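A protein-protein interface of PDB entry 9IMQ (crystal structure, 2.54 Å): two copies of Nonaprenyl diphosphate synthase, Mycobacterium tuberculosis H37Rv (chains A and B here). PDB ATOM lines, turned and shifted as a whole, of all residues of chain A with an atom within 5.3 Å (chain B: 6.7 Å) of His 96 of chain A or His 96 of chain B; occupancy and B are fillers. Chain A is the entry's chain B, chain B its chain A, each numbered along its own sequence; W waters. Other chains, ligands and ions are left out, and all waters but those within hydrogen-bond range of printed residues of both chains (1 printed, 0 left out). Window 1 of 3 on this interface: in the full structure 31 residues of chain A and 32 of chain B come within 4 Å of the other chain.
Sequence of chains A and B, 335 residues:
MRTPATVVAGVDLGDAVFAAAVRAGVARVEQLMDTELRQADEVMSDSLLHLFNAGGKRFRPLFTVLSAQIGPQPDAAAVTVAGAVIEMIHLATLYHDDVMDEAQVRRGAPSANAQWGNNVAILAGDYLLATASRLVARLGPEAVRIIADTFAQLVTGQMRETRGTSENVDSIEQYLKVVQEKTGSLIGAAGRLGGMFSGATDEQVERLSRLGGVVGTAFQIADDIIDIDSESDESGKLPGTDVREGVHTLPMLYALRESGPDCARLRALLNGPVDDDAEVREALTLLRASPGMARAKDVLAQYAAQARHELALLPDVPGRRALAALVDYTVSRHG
Water W1 bridges OD2 of Asp 126 of chain A (3.0 Å) and OE1 of Gln 158 of chain B (3.0 Å).
Of the 21 printed residues of chain B, 6 touch a printed residue of chain A.
Hydrophobic or aromatic side chains of chain B within 4 Å of the printed part of chain A: His 96, Val 99, Met 100 and Ile 122.
Leu 91 of chain A touches none of the printed residues of chain B.
Thr 93 of chain A touches none of the printed residues of chain B.
Of chain B, only His 96, Asn 119, Ile 122 and Asp 126 come within 4 Å of His 96 of chain A.
Of the printed residues of chain B, Asp 126 of chain A touches His 96 (2.6 Å).
Of chain A, only His 96 (3.7 Å), Ile 122 (3.6 Å) and Asp 126 (2.6 Å) come within 4 Å of His 96 of chain B.
Printed residues of chain A within 4 Å of Ile 122 of chain B: His 96 and Ile 122.
The nearest residue of chain B that does not touch His 96 of chain A is Leu 123 of chain B (5.2 Å).
The nearest printed residue of chain B that does not touch Asp 126 of chain A is Asp 126 of chain B (4.3 Å).
His 96 of chain A touches His 96 of chain B.
His 96 of chain A touches Asn 119 of chain B (O to ND2, 3.6 Å).
ND1 of His 96 of chain A touches CG2 of Ile 122 of chain B (3.2 Å).
His 96 of chain B touches Ile 122 of chain A.
Ile 122 of chain A touches Val 99 of chain B (CD1 to CG1, 3.7 Å).
Ile 122 of chain A touches Met 100 of chain B.
Ile 122 of chain B touches Ile 122 of chain A (CD1 to CG1, 3.6 Å).
O of Ile 122 of chain B lies within hydrogen-bond range of NE2 of His 96 of chain B, 2.9 Å away.
A ring nitrogen (NE2) of His 96 of chain B lies close to the side-chain carboxylate (OD1) of Asp 126 of chain B (3.2 Å).
NE2 of His 96 of chain A lies within hydrogen-bond range of O of Ile 122 of chain A, at 3.3 Å.
A ring nitrogen (NE2) of His 96 of chain A lies within hydrogen-bond range of the side-chain carboxylate of Asp 126 of chain A.
ND1 of His 96 of chain B is in hydrogen-bond range of OD2 of Asp 126 of chain A, at 2.6 Å.
The side-chain amide nitrogen (ND2) of Asn 119 of chain B lies within hydrogen-bond range of the backbone carbonyl oxygen (O) of Val 99 of chain A, at 2.6 Å.
The side-chain carboxylate (OD2) of Asp 126 of chain B is in hydrogen-bond range of a ring nitrogen (ND1) of His 96 of chain A (2.7 Å).
His 96 of chain B touches its own counterpart, His 96 of chain A.
His 96 of chain A touches Ile 122 of chain B, and with the chains exchanged Ile 122 of chain A touches His 96 of chain B.
His 96 of chain A touches Asp 126 of chain B, and with the chains exchanged Asp 126 of chain A touches His 96 of chain B.
Ile 122 of chain A touches its own counterpart, Ile 122 of chain B.
Positions printed for both chains: 91, 92, 93, 94, 95, 96, 97, 98, 99, 121, 122, 125, 126 and 129.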
ATOM      1  N   LEU A  91     -18.527  -4.000  11.850  1.00  0.00           N
ATOM      2  CA  LEU A  91     -17.384  -3.219  11.372  1.00  0.00           C
ATOM      3  C   LEU A  91     -16.244  -3.202  12.386  1.00  0.00           C
ATOM      4  O   LEU A  91     -15.076  -3.321  12.011  1.00  0.00           O
ATOM      5  CB  LEU A  91     -17.804  -1.781  11.048  1.00  0.00           C
ATOM      6  CG  LEU A  91     -18.899  -1.509  10.018  1.00  0.00           C
ATOM      7  CD1 LEU A  91     -19.249  -0.025  10.015  1.00  0.00           C
ATOM      8  CD2 LEU A  91     -18.495  -1.987   8.623  1.00  0.00           C
ATOM      9  N   ALA A  92     -16.557  -3.047  13.674  1.00  0.00           N
ATOM     10  CA  ALA A  92     -15.484  -2.965  14.663  1.00  0.00           C
ATOM     11  C   ALA A  92     -14.580  -4.190  14.593  1.00  0.00           C
ATOM     12  O   ALA A  92     -13.350  -4.060  14.680  1.00  0.00           O
ATOM     13  CB  ALA A  92     -16.060  -2.791  16.070  1.00  0.00           C
ATOM     14  N   THR A  93     -15.170  -5.387  14.408  1.00  0.00           N
ATOM     15  CA  THR A  93     -14.368  -6.602  14.257  1.00  0.00           C
ATOM     16  C   THR A  93     -13.553  -6.582  12.965  1.00  0.00           C
ATOM     17  O   THR A  93     -12.492  -7.204  12.891  1.00  0.00           O
ATOM     18  CB  THR A  93     -15.259  -7.841  14.290  1.00  0.00           C
ATOM     19  OG1 THR A  93     -16.102  -7.825  13.138  1.00  0.00           O
ATOM     20  CG2 THR A  93     -16.126  -7.861  15.514  1.00  0.00           C
ATOM     21  N   LEU A  94     -14.021  -5.866  11.944  1.00  0.00           N
ATOM     22  CA  LEU A  94     -13.240  -5.743  10.715  1.00  0.00           C
ATOM     23  C   LEU A  94     -11.985  -4.913  10.942  1.00  0.00           C
ATOM     24  O   LEU A  94     -10.881  -5.303  10.540  1.00  0.00           O
ATOM     25  CB  LEU A  94     -14.094  -5.129   9.606  1.00  0.00           C
ATOM     26  CG  LEU A  94     -15.132  -6.056   8.950  1.00  0.00           C
ATOM     27  CD1 LEU A  94     -15.646  -5.471   7.632  1.00  0.00           C
ATOM     28  CD2 LEU A  94     -14.591  -7.488   8.762  1.00  0.00           C
ATOM     29  N   TYR A  95     -12.141  -3.756  11.583  1.00  0.00           N
ATOM     30  CA  TYR A  95     -10.989  -2.919  11.888  1.00  0.00           C
ATOM     31  C   TYR A  95      -9.988  -3.665  12.748  1.00  0.00           C
ATOM     32  O   TYR A  95      -8.771  -3.559  12.535  1.00  0.00           O
ATOM     33  CB  TYR A  95     -11.444  -1.651  12.591  1.00  0.00           C
ATOM     34  CG  TYR A  95     -11.870  -0.606  11.624  1.00  0.00           C
ATOM     35  CD1 TYR A  95     -10.961  -0.052  10.739  1.00  0.00           C
ATOM     36  CD2 TYR A  95     -13.180  -0.173  11.581  1.00  0.00           C
ATOM     37  CE1 TYR A  95     -11.347   0.917   9.846  1.00  0.00           C
ATOM     38  CE2 TYR A  95     -13.572   0.790  10.689  1.00  0.00           C
ATOM     39  CZ  TYR A  95     -12.652   1.323   9.820  1.00  0.00           C
ATOM     40  OH  TYR A  95     -13.046   2.279   8.920  1.00  0.00           O
ATOM     41  N   HIS A  96     -10.486  -4.449  13.710  1.00  0.00           N
ATOM     42  CA  HIS A  96      -9.591  -5.079  14.668  1.00  0.00           C
ATOM     43  C   HIS A  96      -8.731  -6.154  14.028  1.00  0.00           C
ATOM     44  O   HIS A  96      -7.595  -6.364  14.459  1.00  0.00           O
ATOM     45  CB  HIS A  96     -10.398  -5.632  15.830  1.00  0.00           C
ATOM     46  CG  HIS A  96     -10.616  -4.623  16.904  1.00  0.00           C
ATOM     47  ND1 HIS A  96     -11.053  -4.953  18.172  1.00  0.00           N
ATOM     48  CD2 HIS A  96     -10.430  -3.280  16.903  1.00  0.00           C
ATOM     49  CE1 HIS A  96     -11.140  -3.853  18.898  1.00  0.00           C
ATOM     50  NE2 HIS A  96     -10.774  -2.826  18.150  1.00  0.00           N
ATOM     51  N   ASP A  97      -9.245  -6.832  13.001  1.00  0.00           N
ATOM     52  CA  ASP A  97      -8.470  -7.817  12.253  1.00  0.00           C
ATOM     53  C   ASP A  97      -7.532  -7.190  11.236  1.00  0.00           C
ATOM     54  O   ASP A  97      -6.746  -7.914  10.627  1.00  0.00           O
ATOM     55  CB  ASP A  97      -9.416  -8.789  11.550  1.00  0.00           C
ATOM     56  CG  ASP A  97     -10.455  -9.332  12.491  1.00  0.00           C
ATOM     57  OD1 ASP A  97     -10.349  -8.987  13.703  1.00  0.00           O
ATOM     58  OD2 ASP A  97     -11.367 -10.074  12.038  1.00  0.00           O
ATOM     59  N   ASP A  98      -7.608  -5.880  11.014  1.00  0.00           N
ATOM     60  CA  ASP A  98      -6.576  -5.199  10.246  1.00  0.00           C
ATOM     61  C   ASP A  98      -5.374  -4.818  11.111  1.00  0.00           C
ATOM     62  O   ASP A  98      -4.425  -4.213  10.589  1.00  0.00           O
ATOM     63  CB  ASP A  98      -7.143  -3.951   9.546  1.00  0.00           C
ATOM     64  CG  ASP A  98      -8.204  -4.280   8.496  1.00  0.00           C
ATOM     65  OD1 ASP A  98      -8.219  -5.426   7.973  1.00  0.00           O
ATOM     66  OD2 ASP A  98      -9.032  -3.380   8.191  1.00  0.00           O
ATOM     67  N   VAL A  99      -5.406  -5.141  12.413  1.00  0.00           N
ATOM     68  CA  VAL A  99      -4.218  -5.040  13.254  1.00  0.00           C
ATOM     69  C   VAL A  99      -3.274  -6.182  12.904  1.00  0.00           C
ATOM     70  O   VAL A  99      -3.676  -7.352  12.921  1.00  0.00           O
ATOM     71  CB  VAL A  99      -4.584  -5.087  14.747  1.00  0.00           C
ATOM     72  CG1 VAL A  99      -3.316  -5.062  15.605  1.00  0.00           C
ATOM     73  CG2 VAL A  99      -5.513  -3.963  15.122  1.00  0.00           C
ATOM     74  N   ALA A 121      -6.709   1.163  13.374  1.00  0.00           N
ATOM     75  CA  ALA A 121      -7.530  -0.037  13.464  1.00  0.00           C
ATOM     76  C   ALA A 121      -8.162  -0.163  14.850  1.00  0.00           C
ATOM     77  O   ALA A 121      -9.385  -0.253  14.981  1.00  0.00           O
ATOM     78  CB  ALA A 121      -6.694  -1.266  13.123  1.00  0.00           C
ATOM     79  N   ILE A 122      -7.342  -0.116  15.902  1.00  0.00           N
ATOM     80  CA  ILE A 122      -7.836  -0.360  17.258  1.00  0.00           C
ATOM     81  C   ILE A 122      -8.850   0.707  17.675  1.00  0.00           C
ATOM     82  O   ILE A 122      -9.945   0.397  18.171  1.00  0.00           O
ATOM     83  CB  ILE A 122      -6.656  -0.445  18.242  1.00  0.00           C
ATOM     84  CG1 ILE A 122      -5.683  -1.538  17.783  1.00  0.00           C
ATOM     85  CG2 ILE A 122      -7.158  -0.755  19.650  1.00  0.00           C
ATOM     86  CD1 ILE A 122      -4.255  -1.347  18.241  1.00  0.00           C
ATOM     87  N   GLY A 125     -12.178   0.619  15.588  1.00  0.00           N
ATOM     88  CA  GLY A 125     -12.949  -0.462  16.173  1.00  0.00           C
ATOM     89  C   GLY A 125     -13.443  -0.142  17.571  1.00  0.00           C
ATOM     90  O   GLY A 125     -14.579  -0.467  17.916  1.00  0.00           O
ATOM     91  N   ASP A 126     -12.607   0.521  18.398  1.00  0.00           N
ATOM     92  CA  ASP A 126     -13.052   0.847  19.755  1.00  0.00           C
ATOM     93  C   ASP A 126     -14.109   1.955  19.758  1.00  0.00           C
ATOM     94  O   ASP A 126     -15.069   1.899  20.536  1.00  0.00           O
ATOM     95  CB  ASP A 126     -11.863   1.219  20.633  1.00  0.00           C
ATOM     96  CG  ASP A 126     -11.131   0.001  21.142  1.00  0.00           C
ATOM     97  OD1 ASP A 126     -11.482  -1.102  20.700  1.00  0.00           O
ATOM     98  OD2 ASP A 126     -10.200   0.133  21.957  1.00  0.00           O
ATOM     99  N   LEU A 129     -17.379   0.279  18.927  1.00  0.00           N
ATOM    100  CA  LEU A 129     -17.942  -0.456  20.049  1.00  0.00           C
ATOM    101  C   LEU A 129     -18.508   0.500  21.083  1.00  0.00           C
ATOM    102  O   LEU A 129     -19.545   0.222  21.698  1.00  0.00           O
ATOM    103  CB  LEU A 129     -16.875  -1.364  20.664  1.00  0.00           C
ATOM    104  CG  LEU A 129     -16.297  -2.355  19.645  1.00  0.00           C
ATOM    105  CD1 LEU A 129     -14.949  -2.890  20.079  1.00  0.00           C
ATOM    106  CD2 LEU A 129     -17.274  -3.515  19.377  1.00  0.00           C
ATOM    107  N   LEU B  91      -9.123  -2.841  32.478  1.00  0.00           N
ATOM    108  CA  LEU B  91      -8.225  -3.900  32.024  1.00  0.00           C
ATOM    109  C   LEU B  91      -8.215  -4.003  30.501  1.00  0.00           C
ATOM    110  O   LEU B  91      -7.147  -4.154  29.883  1.00  0.00           O
ATOM    111  CB  LEU B  91      -8.647  -5.225  32.637  1.00  0.00           C
ATOM    112  CG  LEU B  91      -7.888  -5.752  33.838  1.00  0.00           C
ATOM    113  CD1 LEU B  91      -8.180  -7.249  33.953  1.00  0.00           C
ATOM    114  CD2 LEU B  91      -6.400  -5.492  33.698  1.00  0.00           C
ATOM    115  N   ALA B  92      -9.401  -3.945  29.885  1.00  0.00           N
ATOM    116  CA  ALA B  92      -9.500  -3.901  28.431  1.00  0.00           C
ATOM    117  C   ALA B  92      -8.587  -2.838  27.840  1.00  0.00           C
ATOM    118  O   ALA B  92      -7.892  -3.089  26.843  1.00  0.00           O
ATOM    119  CB  ALA B  92     -10.950  -3.647  28.006  1.00  0.00           C
ATOM    120  N   THR B  93      -8.571  -1.642  28.435  1.00  0.00           N
ATOM    121  CA  THR B  93      -7.772  -0.572  27.851  1.00  0.00           C
ATOM    122  C   THR B  93      -6.278  -0.807  28.048  1.00  0.00           C
ATOM    123  O   THR B  93      -5.478  -0.315  27.254  1.00  0.00           O
ATOM    124  CB  THR B  93      -8.194   0.799  28.408  1.00  0.00           C
ATOM    125  OG1 THR B  93      -7.705   0.963  29.745  1.00  0.00           O
ATOM    126  CG2 THR B  93      -9.725   0.955  28.401  1.00  0.00           C
ATOM    127  N   LEU B  94      -5.877  -1.567  29.065  1.00  0.00           N
ATOM    128  CA  LEU B  94      -4.464  -1.921  29.178  1.00  0.00           C
ATOM    129  C   LEU B  94      -4.020  -2.862  28.053  1.00  0.00           C
ATOM    130  O   LEU B  94      -2.915  -2.702  27.512  1.00  0.00           O
ATOM    131  CB  LEU B  94      -4.185  -2.551  30.540  1.00  0.00           C
ATOM    132  CG  LEU B  94      -4.402  -1.723  31.808  1.00  0.00           C
ATOM    133  CD1 LEU B  94      -3.824  -2.481  32.994  1.00  0.00           C
ATOM    134  CD2 LEU B  94      -3.777  -0.312  31.700  1.00  0.00           C
ATOM    135  N   TYR B  95      -4.853  -3.856  27.692  1.00  0.00           N
ATOM    136  CA  TYR B  95      -4.565  -4.674  26.511  1.00  0.00           C
ATOM    137  C   TYR B  95      -4.444  -3.806  25.269  1.00  0.00           C
ATOM    138  O   TYR B  95      -3.501  -3.950  24.482  1.00  0.00           O
ATOM    139  CB  TYR B  95      -5.646  -5.734  26.295  1.00  0.00           C
ATOM    140  CG  TYR B  95      -5.583  -6.870  27.284  1.00  0.00           C
ATOM    141  CD1 TYR B  95      -6.146  -6.741  28.555  1.00  0.00           C
ATOM    142  CD2 TYR B  95      -4.961  -8.058  26.966  1.00  0.00           C
ATOM    143  CE1 TYR B  95      -6.079  -7.758  29.477  1.00  0.00           C
ATOM    144  CE2 TYR B  95      -4.896  -9.104  27.888  1.00  0.00           C
ATOM    145  CZ  TYR B  95      -5.454  -8.946  29.146  1.00  0.00           C
ATOM    146  OH  TYR B  95      -5.395  -9.976  30.070  1.00  0.00           O
ATOM    147  N   HIS B  96      -5.388  -2.882  25.081  1.00  0.00           N
ATOM    148  CA  HIS B  96      -5.383  -2.067  23.874  1.00  0.00           C
ATOM    149  C   HIS B  96      -4.247  -1.039  23.886  1.00  0.00           C
ATOM    150  O   HIS B  96      -3.548  -0.864  22.877  1.00  0.00           O
ATOM    151  CB  HIS B  96      -6.758  -1.432  23.712  1.00  0.00           C
ATOM    152  CG  HIS B  96      -7.777  -2.401  23.202  1.00  0.00           C
ATOM    153  ND1 HIS B  96      -8.910  -2.018  22.510  1.00  0.00           N
ATOM    154  CD2 HIS B  96      -7.801  -3.758  23.240  1.00  0.00           C
ATOM    155  CE1 HIS B  96      -9.591  -3.096  22.160  1.00  0.00           C
ATOM    156  NE2 HIS B  96      -8.936  -4.164  22.586  1.00  0.00           N
ATOM    157  N   ASP B  97      -4.025  -0.375  25.028  1.00  0.00           N
ATOM    158  CA  ASP B  97      -2.905   0.552  25.143  1.00  0.00           C
ATOM    159  C   ASP B  97      -1.578  -0.145  24.854  1.00  0.00           C
ATOM    160  O   ASP B  97      -0.745   0.367  24.090  1.00  0.00           O
ATOM    161  CB  ASP B  97      -2.883   1.185  26.537  1.00  0.00           C
ATOM    162  CG  ASP B  97      -4.005   2.185  26.741  1.00  0.00           C
ATOM    163  OD1 ASP B  97      -4.512   2.671  25.706  1.00  0.00           O
ATOM    164  OD2 ASP B  97      -4.381   2.464  27.918  1.00  0.00           O
ATOM    165  N   ASP B  98      -1.369  -1.330  25.442  1.00  0.00           N
ATOM    166  CA  ASP B  98      -0.078  -1.998  25.293  1.00  0.00           C
ATOM    167  C   ASP B  98       0.193  -2.427  23.851  1.00  0.00           C
ATOM    168  O   ASP B  98       1.355  -2.436  23.424  1.00  0.00           O
ATOM    169  CB  ASP B  98       0.016  -3.167  26.274  1.00  0.00           C
ATOM    170  CG  ASP B  98       0.260  -2.676  27.712  1.00  0.00           C
ATOM    171  OD1 ASP B  98       0.614  -1.478  27.851  1.00  0.00           O
ATOM    172  OD2 ASP B  98       0.095  -3.452  28.687  1.00  0.00           O
ATOM    173  N   VAL B  99      -0.846  -2.736  23.071  1.00  0.00           N
ATOM    174  CA  VAL B  99      -0.643  -2.934  21.636  1.00  0.00           C
ATOM    175  C   VAL B  99      -0.348  -1.602  20.946  1.00  0.00           C
ATOM    176  O   VAL B  99       0.544  -1.510  20.096  1.00  0.00           O
ATOM    177  CB  VAL B  99      -1.862  -3.639  21.016  1.00  0.00           C
ATOM    178  CG1 VAL B  99      -1.741  -3.682  19.492  1.00  0.00           C
ATOM    179  CG2 VAL B  99      -1.995  -5.034  21.577  1.00  0.00           C
ATOM    180  N   MET B 100      -1.084  -0.548  21.302  1.00  0.00           N
ATOM    181  CA  MET B 100      -0.893   0.738  20.636  1.00  0.00           C
ATOM    182  C   MET B 100       0.490   1.317  20.928  1.00  0.00           C
ATOM    183  O   MET B 100       1.194   1.750  20.013  1.00  0.00           O
ATOM    184  CB  MET B 100      -1.997   1.713  21.053  1.00  0.00           C
ATOM    185  CG  MET B 100      -3.102   1.857  20.024  1.00  0.00           C
ATOM    186  SD  MET B 100      -4.563   2.742  20.606  1.00  0.00           S
ATOM    187  CE  MET B 100      -4.877   1.955  22.192  1.00  0.00           C
ATOM    188  N   ASP B 101       0.892   1.347  22.197  1.00  0.00           N
ATOM    189  CA  ASP B 101       2.209   1.841  22.582  1.00  0.00           C
ATOM    190  C   ASP B 101       3.317   0.838  22.281  1.00  0.00           C
ATOM    191  O   ASP B 101       4.446   1.041  22.742  1.00  0.00           O
ATOM    192  CB  ASP B 101       2.232   2.193  24.076  1.00  0.00           C
ATOM    193  CG  ASP B 101       1.123   3.176  24.478  1.00  0.00           C
ATOM    194  OD1 ASP B 101       0.886   4.174  23.748  1.00  0.00           O
ATOM    195  OD2 ASP B 101       0.495   2.951  25.538  1.00  0.00           O
ATOM    196  N   ASN B 119      -2.896  -9.324  17.841  1.00  0.00           N
ATOM    197  CA  ASN B 119      -4.287  -9.689  17.622  1.00  0.00           C
ATOM    198  C   ASN B 119      -4.859 -10.435  18.819  1.00  0.00           C
ATOM    199  O   ASN B 119      -6.008 -10.202  19.204  1.00  0.00           O
ATOM    200  CB  ASN B 119      -4.424 -10.503  16.330  1.00  0.00           C
ATOM    201  CG  ASN B 119      -4.097  -9.672  15.090  1.00  0.00           C
ATOM    202  OD1 ASN B 119      -3.180  -9.991  14.335  1.00  0.00           O
ATOM    203  ND2 ASN B 119      -4.834  -8.581  14.899  1.00  0.00           N
ATOM    204  N   ALA B 121      -4.017  -9.962  21.801  1.00  0.00           N
ATOM    205  CA  ALA B 121      -4.183  -8.916  22.800  1.00  0.00           C
ATOM    206  C   ALA B 121      -5.437  -8.095  22.527  1.00  0.00           C
ATOM    207  O   ALA B 121      -6.260  -7.875  23.428  1.00  0.00           O
ATOM    208  CB  ALA B 121      -2.950  -8.028  22.808  1.00  0.00           C
ATOM    209  N   ILE B 122      -5.604  -7.637  21.284  1.00  0.00           N
ATOM    210  CA  ILE B 122      -6.760  -6.814  20.965  1.00  0.00           C
ATOM    211  C   ILE B 122      -8.034  -7.560  21.302  1.00  0.00           C
ATOM    212  O   ILE B 122      -8.960  -6.999  21.905  1.00  0.00           O
ATOM    213  CB  ILE B 122      -6.736  -6.382  19.490  1.00  0.00           C
ATOM    214  CG1 ILE B 122      -5.540  -5.458  19.218  1.00  0.00           C
ATOM    215  CG2 ILE B 122      -8.049  -5.687  19.137  1.00  0.00           C
ATOM    216  CD1 ILE B 122      -5.432  -4.242  20.173  1.00  0.00           C
ATOM    217  N   LEU B 123      -8.087  -8.847  20.951  1.00  0.00           N
ATOM    218  CA  LEU B 123      -9.288  -9.640  21.171  1.00  0.00           C
ATOM    219  C   LEU B 123      -9.562  -9.830  22.657  1.00  0.00           C
ATOM    220  O   LEU B 123     -10.706  -9.703  23.113  1.00  0.00           O
ATOM    221  CB  LEU B 123      -9.142 -10.978  20.460  1.00  0.00           C
ATOM    222  CG  LEU B 123      -9.047 -10.878  18.937  1.00  0.00           C
ATOM    223  CD1 LEU B 123      -8.746 -12.247  18.296  1.00  0.00           C
ATOM    224  CD2 LEU B 123     -10.304 -10.224  18.325  1.00  0.00           C
ATOM    225  N   ALA B 124      -8.520 -10.163  23.418  1.00  0.00           N
ATOM    226  CA  ALA B 124      -8.608 -10.237  24.875  1.00  0.00           C
ATOM    227  C   ALA B 124      -9.282  -9.001  25.473  1.00  0.00           C
ATOM    228  O   ALA B 124     -10.192  -9.113  26.303  1.00  0.00           O
ATOM    229  CB  ALA B 124      -7.201 -10.414  25.452  1.00  0.00           C
ATOM    230  N   GLY B 125      -8.828  -7.809  25.079  1.00  0.00           N
ATOM    231  CA  GLY B 125      -9.476  -6.591  25.543  1.00  0.00           C
ATOM    232  C   GLY B 125     -10.934  -6.514  25.132  1.00  0.00           C
ATOM    233  O   GLY B 125     -11.806  -6.189  25.946  1.00  0.00           O
ATOM    234  N   ASP B 126     -11.216  -6.819  23.866  1.00  0.00           N
ATOM    235  CA  ASP B 126     -12.590  -6.917  23.387  1.00  0.00           C
ATOM    236  C   ASP B 126     -13.434  -7.801  24.286  1.00  0.00           C
ATOM    237  O   ASP B 126     -14.579  -7.471  24.616  1.00  0.00           O
ATOM    238  CB  ASP B 126     -12.596  -7.483  21.973  1.00  0.00           C
ATOM    239  CG  ASP B 126     -12.123  -6.489  20.947  1.00  0.00           C
ATOM    240  OD1 ASP B 126     -11.646  -5.388  21.334  1.00  0.00           O
ATOM    241  OD2 ASP B 126     -12.214  -6.829  19.751  1.00  0.00           O
ATOM    242  N   TYR B 127     -12.901  -8.955  24.655  1.00  0.00           N
ATOM    243  CA  TYR B 127     -13.694  -9.882  25.453  1.00  0.00           C
ATOM    244  C   TYR B 127     -13.959  -9.320  26.842  1.00  0.00           C
ATOM    245  O   TYR B 127     -14.983  -9.639  27.463  1.00  0.00           O
ATOM    246  CB  TYR B 127     -12.978 -11.232  25.533  1.00  0.00           C
ATOM    247  CG  TYR B 127     -13.858 -12.310  26.088  1.00  0.00           C
ATOM    248  CD1 TYR B 127     -13.982 -12.493  27.462  1.00  0.00           C
ATOM    249  CD2 TYR B 127     -14.593 -13.134  25.243  1.00  0.00           C
ATOM    250  CE1 TYR B 127     -14.811 -13.483  27.976  1.00  0.00           C
ATOM    251  CE2 TYR B 127     -15.412 -14.116  25.748  1.00  0.00           C
ATOM    252  CZ  TYR B 127     -15.521 -14.284  27.111  1.00  0.00           C
ATOM    253  OH  TYR B 127     -16.348 -15.261  27.610  1.00  0.00           O
ATOM    254  N   LEU B 129     -14.433  -6.096  27.311  1.00  0.00           N
ATOM    255  CA  LEU B 129     -15.490  -5.121  27.072  1.00  0.00           C
ATOM    256  C   LEU B 129     -16.857  -5.799  27.031  1.00  0.00           C
ATOM    257  O   LEU B 129     -17.833  -5.280  27.587  1.00  0.00           O
ATOM    258  CB  LEU B 129     -15.207  -4.348  25.775  1.00  0.00           C
ATOM    259  CG  LEU B 129     -13.940  -3.452  25.724  1.00  0.00           C
ATOM    260  CD1 LEU B 129     -13.623  -2.919  24.322  1.00  0.00           C
ATOM    261  CD2 LEU B 129     -13.986  -2.271  26.728  1.00  0.00           C
ATOM    262  N   GLN B 158      -8.743   8.697  24.046  1.00  0.00           N
ATOM    263  CA  GLN B 158      -7.701   7.985  23.308  1.00  0.00           C
ATOM    264  C   GLN B 158      -7.532   8.549  21.889  1.00  0.00           C
ATOM    265  O   GLN B 158      -6.404   8.751  21.419  1.00  0.00           O
ATOM    266  CB  GLN B 158      -8.020   6.485  23.262  1.00  0.00           C
ATOM    267  CG  GLN B 158      -7.932   5.711  24.597  1.00  0.00           C
ATOM    268  CD  GLN B 158      -8.435   4.234  24.510  1.00  0.00           C
ATOM    269  OE1 GLN B 158      -9.580   3.964  24.112  1.00  0.00           O
ATOM    270  NE2 GLN B 158      -7.578   3.288  24.909  1.00  0.00           N
HETATM  271  O   HOH W   1      -9.620   1.029  24.729  1.00  0.00           O
